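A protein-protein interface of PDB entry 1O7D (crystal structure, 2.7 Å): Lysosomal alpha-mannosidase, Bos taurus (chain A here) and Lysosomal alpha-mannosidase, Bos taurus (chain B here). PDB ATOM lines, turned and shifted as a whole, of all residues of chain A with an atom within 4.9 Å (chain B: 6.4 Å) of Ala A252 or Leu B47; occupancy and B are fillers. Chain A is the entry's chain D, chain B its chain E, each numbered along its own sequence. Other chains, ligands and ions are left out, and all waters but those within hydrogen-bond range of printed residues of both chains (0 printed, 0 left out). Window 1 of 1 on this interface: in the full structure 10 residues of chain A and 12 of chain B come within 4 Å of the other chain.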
ATOM      1  N   THR A 249      15.423  25.450 -13.152  1.00  0.00           N
ATOM      2  CA  THR A 249      14.334  24.529 -12.801  1.00  0.00           C
ATOM      3  C   THR A 249      14.013  24.511 -11.295  1.00  0.00           C
ATOM      4  O   THR A 249      12.990  23.955 -10.869  1.00  0.00           O
ATOM      5  CB  THR A 249      14.698  23.088 -13.251  1.00  0.00           C
ATOM      6  OG1 THR A 249      14.842  23.069 -14.672  1.00  0.00           O
ATOM      7  CG2 THR A 249      13.623  22.085 -12.856  1.00  0.00           C
ATOM      8  N   ALA A 250      14.880  25.127 -10.495  1.00  0.00           N
ATOM      9  CA  ALA A 250      14.703  25.142  -9.049  1.00  0.00           C
ATOM     10  C   ALA A 250      13.371  25.717  -8.550  1.00  0.00           C
ATOM     11  O   ALA A 250      12.652  25.075  -7.777  1.00  0.00           O
ATOM     12  CB  ALA A 250      15.863  25.888  -8.400  1.00  0.00           C
ATOM     13  N   ALA A 251      13.051  26.921  -9.003  1.00  0.00           N
ATOM     14  CA  ALA A 251      11.851  27.621  -8.578  1.00  0.00           C
ATOM     15  C   ALA A 251      10.613  26.771  -8.394  1.00  0.00           C
ATOM     16  O   ALA A 251      10.053  26.711  -7.303  1.00  0.00           O
ATOM     17  CB  ALA A 251      11.553  28.728  -9.537  1.00  0.00           C
ATOM     18  N   ALA A 252      10.175  26.126  -9.466  1.00  0.00           N
ATOM     19  CA  ALA A 252       8.970  25.316  -9.412  1.00  0.00           C
ATOM     20  C   ALA A 252       9.002  24.244  -8.327  1.00  0.00           C
ATOM     21  O   ALA A 252       7.986  23.982  -7.680  1.00  0.00           O
ATOM     22  CB  ALA A 252       8.705  24.688 -10.773  1.00  0.00           C
ATOM     23  N   ARG A 253      10.159  23.628  -8.120  1.00  0.00           N
ATOM     24  CA  ARG A 253      10.269  22.595  -7.102  1.00  0.00           C
ATOM     25  C   ARG A 253      10.153  23.124  -5.670  1.00  0.00           C
ATOM     26  O   ARG A 253       9.396  22.570  -4.879  1.00  0.00           O
ATOM     27  CB  ARG A 253      11.593  21.831  -7.235  1.00  0.00           C
ATOM     28  CG  ARG A 253      11.812  21.102  -8.554  1.00  0.00           C
ATOM     29  CD  ARG A 253      10.942  19.875  -8.706  1.00  0.00           C
ATOM     30  NE  ARG A 253      11.152  19.276 -10.020  1.00  0.00           N
ATOM     31  CZ  ARG A 253      10.653  18.103 -10.415  1.00  0.00           C
ATOM     32  NH1 ARG A 253       9.903  17.374  -9.589  1.00  0.00           N
ATOM     33  NH2 ARG A 253      10.885  17.665 -11.651  1.00  0.00           N
ATOM     34  N   HIS A 254      10.883  24.178  -5.305  1.00  0.00           N
ATOM     35  CA  HIS A 254      10.772  24.632  -3.926  1.00  0.00           C
ATOM     36  C   HIS A 254       9.419  25.256  -3.633  1.00  0.00           C
ATOM     37  O   HIS A 254       8.927  25.170  -2.508  1.00  0.00           O
ATOM     38  CB  HIS A 254      11.942  25.557  -3.523  1.00  0.00           C
ATOM     39  CG  HIS A 254      11.873  26.945  -4.078  1.00  0.00           C
ATOM     40  ND1 HIS A 254      10.913  27.858  -3.693  1.00  0.00           N
ATOM     41  CD2 HIS A 254      12.691  27.600  -4.938  1.00  0.00           C
ATOM     42  CE1 HIS A 254      11.145  29.015  -4.289  1.00  0.00           C
ATOM     43  NE2 HIS A 254      12.217  28.885  -5.050  1.00  0.00           N
ATOM     44  N   ARG A 255       8.796  25.848  -4.646  1.00  0.00           N
ATOM     45  CA  ARG A 255       7.477  26.434  -4.456  1.00  0.00           C
ATOM     46  C   ARG A 255       6.478  25.330  -4.112  1.00  0.00           C
ATOM     47  O   ARG A 255       5.859  25.336  -3.046  1.00  0.00           O
ATOM     48  CB  ARG A 255       6.992  27.133  -5.732  1.00  0.00           C
ATOM     49  CG  ARG A 255       7.634  28.482  -6.050  1.00  0.00           C
ATOM     50  CD  ARG A 255       7.488  29.462  -4.892  1.00  0.00           C
ATOM     51  NE  ARG A 255       7.712  30.834  -5.320  1.00  0.00           N
ATOM     52  CZ  ARG A 255       7.969  31.842  -4.494  1.00  0.00           C
ATOM     53  NH1 ARG A 255       8.035  31.620  -3.196  1.00  0.00           N
ATOM     54  NH2 ARG A 255       8.163  33.071  -4.965  1.00  0.00           N
ATOM     55  N   LEU A 256       6.328  24.381  -5.027  1.00  0.00           N
ATOM     56  CA  LEU A 256       5.384  23.279  -4.847  1.00  0.00           C
ATOM     57  C   LEU A 256       5.590  22.379  -3.638  1.00  0.00           C
ATOM     58  O   LEU A 256       4.616  21.894  -3.058  1.00  0.00           O
ATOM     59  CB  LEU A 256       5.348  22.405  -6.099  1.00  0.00           C
ATOM     60  CG  LEU A 256       4.878  23.116  -7.360  1.00  0.00           C
ATOM     61  CD1 LEU A 256       4.901  22.161  -8.527  1.00  0.00           C
ATOM     62  CD2 LEU A 256       3.479  23.663  -7.132  1.00  0.00           C
ATOM     63  N   PRO B  14      -1.177  23.601 -11.079  1.00  0.00           N
ATOM     64  CA  PRO B  14       0.018  23.764 -10.243  1.00  0.00           C
ATOM     65  C   PRO B  14       0.381  25.175  -9.754  1.00  0.00           C
ATOM     66  O   PRO B  14       0.775  25.342  -8.594  1.00  0.00           O
ATOM     67  CB  PRO B  14       1.120  23.137 -11.096  1.00  0.00           C
ATOM     68  CG  PRO B  14       0.589  23.254 -12.495  1.00  0.00           C
ATOM     69  CD  PRO B  14      -0.840  22.888 -12.319  1.00  0.00           C
ATOM     70  N   SER B  15       0.242  26.183 -10.619  1.00  0.00           N
ATOM     71  CA  SER B  15       0.588  27.559 -10.241  1.00  0.00           C
ATOM     72  C   SER B  15      -0.364  28.254  -9.272  1.00  0.00           C
ATOM     73  O   SER B  15      -0.106  29.386  -8.871  1.00  0.00           O
ATOM     74  CB  SER B  15       0.762  28.428 -11.492  1.00  0.00           C
ATOM     75  OG  SER B  15      -0.150  28.047 -12.500  1.00  0.00           O
ATOM     76  N   HIS B  35      -1.716  32.882  -6.276  1.00  0.00           N
ATOM     77  CA  HIS B  35      -0.889  32.379  -7.345  1.00  0.00           C
ATOM     78  C   HIS B  35       0.531  32.234  -6.768  1.00  0.00           C
ATOM     79  O   HIS B  35       1.333  33.149  -6.820  1.00  0.00           O
ATOM     80  CB  HIS B  35      -0.994  33.379  -8.487  1.00  0.00           C
ATOM     81  CG  HIS B  35      -0.180  33.022  -9.680  1.00  0.00           C
ATOM     82  ND1 HIS B  35       1.189  33.156  -9.710  1.00  0.00           N
ATOM     83  CD2 HIS B  35      -0.539  32.559 -10.898  1.00  0.00           C
ATOM     84  CE1 HIS B  35       1.640  32.798 -10.896  1.00  0.00           C
ATOM     85  NE2 HIS B  35       0.611  32.431 -11.637  1.00  0.00           N
ATOM     86  N   PHE B  37       3.397  31.595  -7.458  1.00  0.00           N
ATOM     87  CA  PHE B  37       4.654  31.806  -8.177  1.00  0.00           C
ATOM     88  C   PHE B  37       4.882  33.290  -8.427  1.00  0.00           C
ATOM     89  O   PHE B  37       3.953  34.007  -8.793  1.00  0.00           O
ATOM     90  CB  PHE B  37       4.681  31.050  -9.516  1.00  0.00           C
ATOM     91  CG  PHE B  37       4.834  29.551  -9.379  1.00  0.00           C
ATOM     92  CD1 PHE B  37       6.096  28.947  -9.287  1.00  0.00           C
ATOM     93  CD2 PHE B  37       3.705  28.736  -9.342  1.00  0.00           C
ATOM     94  CE1 PHE B  37       6.217  27.563  -9.164  1.00  0.00           C
ATOM     95  CE2 PHE B  37       3.821  27.356  -9.216  1.00  0.00           C
ATOM     96  CZ  PHE B  37       5.081  26.773  -9.127  1.00  0.00           C
ATOM     97  N   GLU B  41       9.838  32.654 -11.734  1.00  0.00           N
ATOM     98  CA  GLU B  41       9.932  31.267 -11.327  1.00  0.00           C
ATOM     99  C   GLU B  41       9.289  30.292 -12.286  1.00  0.00           C
ATOM    100  O   GLU B  41       8.934  29.179 -11.895  1.00  0.00           O
ATOM    101  CB  GLU B  41       9.323  31.113  -9.950  1.00  0.00           C
ATOM    102  CG  GLU B  41       9.917  32.079  -8.968  1.00  0.00           C
ATOM    103  CD  GLU B  41       9.193  32.056  -7.657  1.00  0.00           C
ATOM    104  OE1 GLU B  41       7.937  31.970  -7.700  1.00  0.00           O
ATOM    105  OE2 GLU B  41       9.879  32.133  -6.606  1.00  0.00           O
ATOM    106  N   ASP B  42       9.148  30.704 -13.541  1.00  0.00           N
ATOM    107  CA  ASP B  42       8.539  29.860 -14.568  1.00  0.00           C
ATOM    108  C   ASP B  42       9.144  28.465 -14.599  1.00  0.00           C
ATOM    109  O   ASP B  42       8.452  27.494 -14.913  1.00  0.00           O
ATOM    110  CB  ASP B  42       8.729  30.492 -15.939  1.00  0.00           C
ATOM    111  CG  ASP B  42       8.130  31.867 -16.028  1.00  0.00           C
ATOM    112  OD1 ASP B  42       6.959  31.972 -16.455  1.00  0.00           O
ATOM    113  OD2 ASP B  42       8.825  32.842 -15.661  1.00  0.00           O
ATOM    114  N   SER B  43      10.441  28.389 -14.286  1.00  0.00           N
ATOM    115  CA  SER B  43      11.186  27.130 -14.270  1.00  0.00           C
ATOM    116  C   SER B  43      11.005  26.318 -15.547  1.00  0.00           C
ATOM    117  O   SER B  43      10.994  25.089 -15.515  1.00  0.00           O
ATOM    118  CB  SER B  43      10.789  26.285 -13.057  1.00  0.00           C
ATOM    119  OG  SER B  43      11.608  26.594 -11.934  1.00  0.00           O
ATOM    120  N   GLY B  44      10.866  27.020 -16.670  1.00  0.00           N
ATOM    121  CA  GLY B  44      10.693  26.359 -17.952  1.00  0.00           C
ATOM    122  C   GLY B  44       9.310  25.788 -18.268  1.00  0.00           C
ATOM    123  O   GLY B  44       9.141  25.116 -19.288  1.00  0.00           O
ATOM    124  N   ARG B  45       8.312  26.047 -17.427  1.00  0.00           N
ATOM    125  CA  ARG B  45       6.985  25.508 -17.681  1.00  0.00           C
ATOM    126  C   ARG B  45       5.915  26.582 -17.624  1.00  0.00           C
ATOM    127  O   ARG B  45       4.783  26.295 -17.228  1.00  0.00           O
ATOM    128  CB  ARG B  45       6.647  24.407 -16.656  1.00  0.00           C
ATOM    129  CG  ARG B  45       7.418  23.081 -16.828  1.00  0.00           C
ATOM    130  CD  ARG B  45       7.084  22.037 -15.742  1.00  0.00           C
ATOM    131  NE  ARG B  45       7.497  22.473 -14.405  1.00  0.00           N
ATOM    132  CZ  ARG B  45       7.283  21.793 -13.272  1.00  0.00           C
ATOM    133  NH1 ARG B  45       6.656  20.624 -13.296  1.00  0.00           N
ATOM    134  NH2 ARG B  45       7.684  22.288 -12.099  1.00  0.00           N
ATOM    135  N   ASN B  46       6.254  27.812 -18.009  1.00  0.00           N
ATOM    136  CA  ASN B  46       5.277  28.902 -17.974  1.00  0.00           C
ATOM    137  C   ASN B  46       4.434  28.748 -16.706  1.00  0.00           C
ATOM    138  O   ASN B  46       3.208  28.728 -16.782  1.00  0.00           O
ATOM    139  CB  ASN B  46       4.333  28.848 -19.199  1.00  0.00           C
ATOM    140  CG  ASN B  46       5.067  28.978 -20.544  1.00  0.00           C
ATOM    141  OD1 ASN B  46       6.000  29.777 -20.684  1.00  0.00           O
ATOM    142  ND2 ASN B  46       4.627  28.201 -21.546  1.00  0.00           N
ATOM    143  N   LEU B  47       5.079  28.605 -15.552  1.00  0.00           N
ATOM    144  CA  LEU B  47       4.351  28.444 -14.295  1.00  0.00           C
ATOM    145  C   LEU B  47       4.096  29.805 -13.682  1.00  0.00           C
ATOM    146  O   LEU B  47       3.287  29.952 -12.772  1.00  0.00           O
ATOM    147  CB  LEU B  47       5.146  27.578 -13.318  1.00  0.00           C
ATOM    148  CG  LEU B  47       5.054  26.064 -13.519  1.00  0.00           C
ATOM    149  CD1 LEU B  47       6.125  25.380 -12.691  1.00  0.00           C
ATOM    150  CD2 LEU B  47       3.675  25.553 -13.102  1.00  0.00           C
ATOM    151  N   SER B  48       4.802  30.801 -14.195  1.00  0.00           N
ATOM    152  CA  SER B  48       4.669  32.177 -13.719  1.00  0.00           C
ATOM    153  C   SER B  48       3.633  32.965 -14.533  1.00  0.00           C
ATOM    154  O   SER B  48       3.279  34.083 -14.177  1.00  0.00           O
ATOM    155  CB  SER B  48       6.028  32.901 -13.787  1.00  0.00           C
ATOM    156  OG  SER B  48       6.594  33.081 -12.501  1.00  0.00           O
ATOM    157  N   SER B  49       3.161  32.381 -15.626  1.00  0.00           N
ATOM    158  CA  SER B  49       2.177  33.042 -16.468  1.00  0.00           C
ATOM    159  C   SER B  49       0.859  33.148 -15.712  1.00  0.00           C
ATOM    160  O   SER B  49       0.615  32.379 -14.778  1.00  0.00           O
ATOM    161  CB  SER B  49       1.964  32.241 -17.758  1.00  0.00           C
ATOM    162  OG  SER B  49       3.122  32.251 -18.576  1.00  0.00           O
ATOM    163  N   PRO B  50       0.000  34.112 -16.094  1.00  0.00           N
ATOM    164  CA  PRO B  50      -1.302  34.312 -15.451  1.00  0.00           C
ATOM    165  C   PRO B  50      -2.176  33.090 -15.694  1.00  0.00           C
ATOM    166  O   PRO B  50      -1.956  32.327 -16.645  1.00  0.00           O
ATOM    167  CB  PRO B  50      -1.860  35.533 -16.159  1.00  0.00           C
ATOM    168  CG  PRO B  50      -0.627  36.266 -16.582  1.00  0.00           C
ATOM    169  CD  PRO B  50       0.251  35.167 -17.087  1.00  0.00           C
ATOM    170  N   VAL B  51      -3.166  32.905 -14.830  1.00  0.00           N
ATOM    171  CA  VAL B  51      -4.074  31.774 -14.941  1.00  0.00           C
ATOM    172  C   VAL B  51      -5.519  32.224 -14.779  1.00  0.00           C
ATOM    173  O   VAL B  51      -5.834  33.077 -13.960  1.00  0.00           O
ATOM    174  CB  VAL B  51      -3.762  30.715 -13.881  1.00  0.00           C
ATOM    175  CG1 VAL B  51      -2.295  30.359 -13.928  1.00  0.00           C
ATOM    176  CG2 VAL B  51      -4.130  31.233 -12.516  1.00  0.00           C
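O of Thr A249 sits at hydrogen-bond distance from OG of Ser B43, 3.2 Å away. The backbone NH (N) of Ala A251 lies close to the side-chain hydroxyl (OG) of Ser B43, at 3.3 Å. The backbone NH (N) of Ala A252 sits at hydrogen-bond distance from the side-chain hydroxyl (OG) of Ser B43 (2.9 Å). OE2 of Glu B41 is in salt-bridge range of NH2 of Arg A255 (2.6 Å).
O of Phe B37 is in hydrogen-bond range of ND1 of His B35. The backbone NH of Glu B41 sits at hydrogen-bond distance from the side-chain hydroxyl of Ser B48, at 3.4 Å.
Among the printed residues, pairs that only touch across the chains: Ala A252 with Arg B45 (2.9 Å), Ala A252 with Leu B47 (3.3 Å), Ala A251 with Glu B41 (3.3 Å), Leu A256 with Pro B14 (3.5 Å), Arg A255 with Phe B37 (3.5 Å), Ala A252 with Phe B37 (3.6 Å) and Ala A250 with Ser B43 (3.9 Å).
Leu B47 touches just one residue of chain A: Ala A252. Printed residues of chain A within 4 Å of Glu B41: Ala A251 and Arg A255. Printed residues of chain B within 4 Å of Thr A249: Ser B43. Printed residues of chain B within 4 Å of Arg A255: Phe B37 and Glu B41. Printed residues of chain B within 4 Å of Ala A250: Ser B43. Printed residues of chain A within 4 Å of Phe B37: Ala A252 (3.6 Å) and Arg A255 (3.5 Å). Val B51 touches none of the printed residues of chain A. The nearest residue of chain B that does not touch Ala A252 is Glu B41 (4.1 Å). The nearest printed residue of chain A that does not touch Leu B47 is Leu A256 (5.4 Å). The nearest printed residue of chain B that does not touch Thr A249 is Arg B45 (5.7 Å).
Of the 15 printed residues of chain B, 6 touch a printed residue of chain A. Printed residues of chain B that touch a printed residue of chain A: Pro B14, Phe B37, Glu B41, Ser B43, Arg B45 and Leu B47. Hydrophobic or aromatic side chains of chain B that line the printed part of chain A: Phe B37 and Leu B47. Hydrophobic or aromatic side chains of chain A that line the printed part of chain B: Ala A251, Ala A252 and Leu A256. Among the printed residues, 11 pairs touch across the chains. Among the printed residues, Asp or Glu carboxylates within 4 Å of a Lys or Arg side-chain nitrogen of the other chain: Arg A255 with Glu B41 (2.6 Å).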
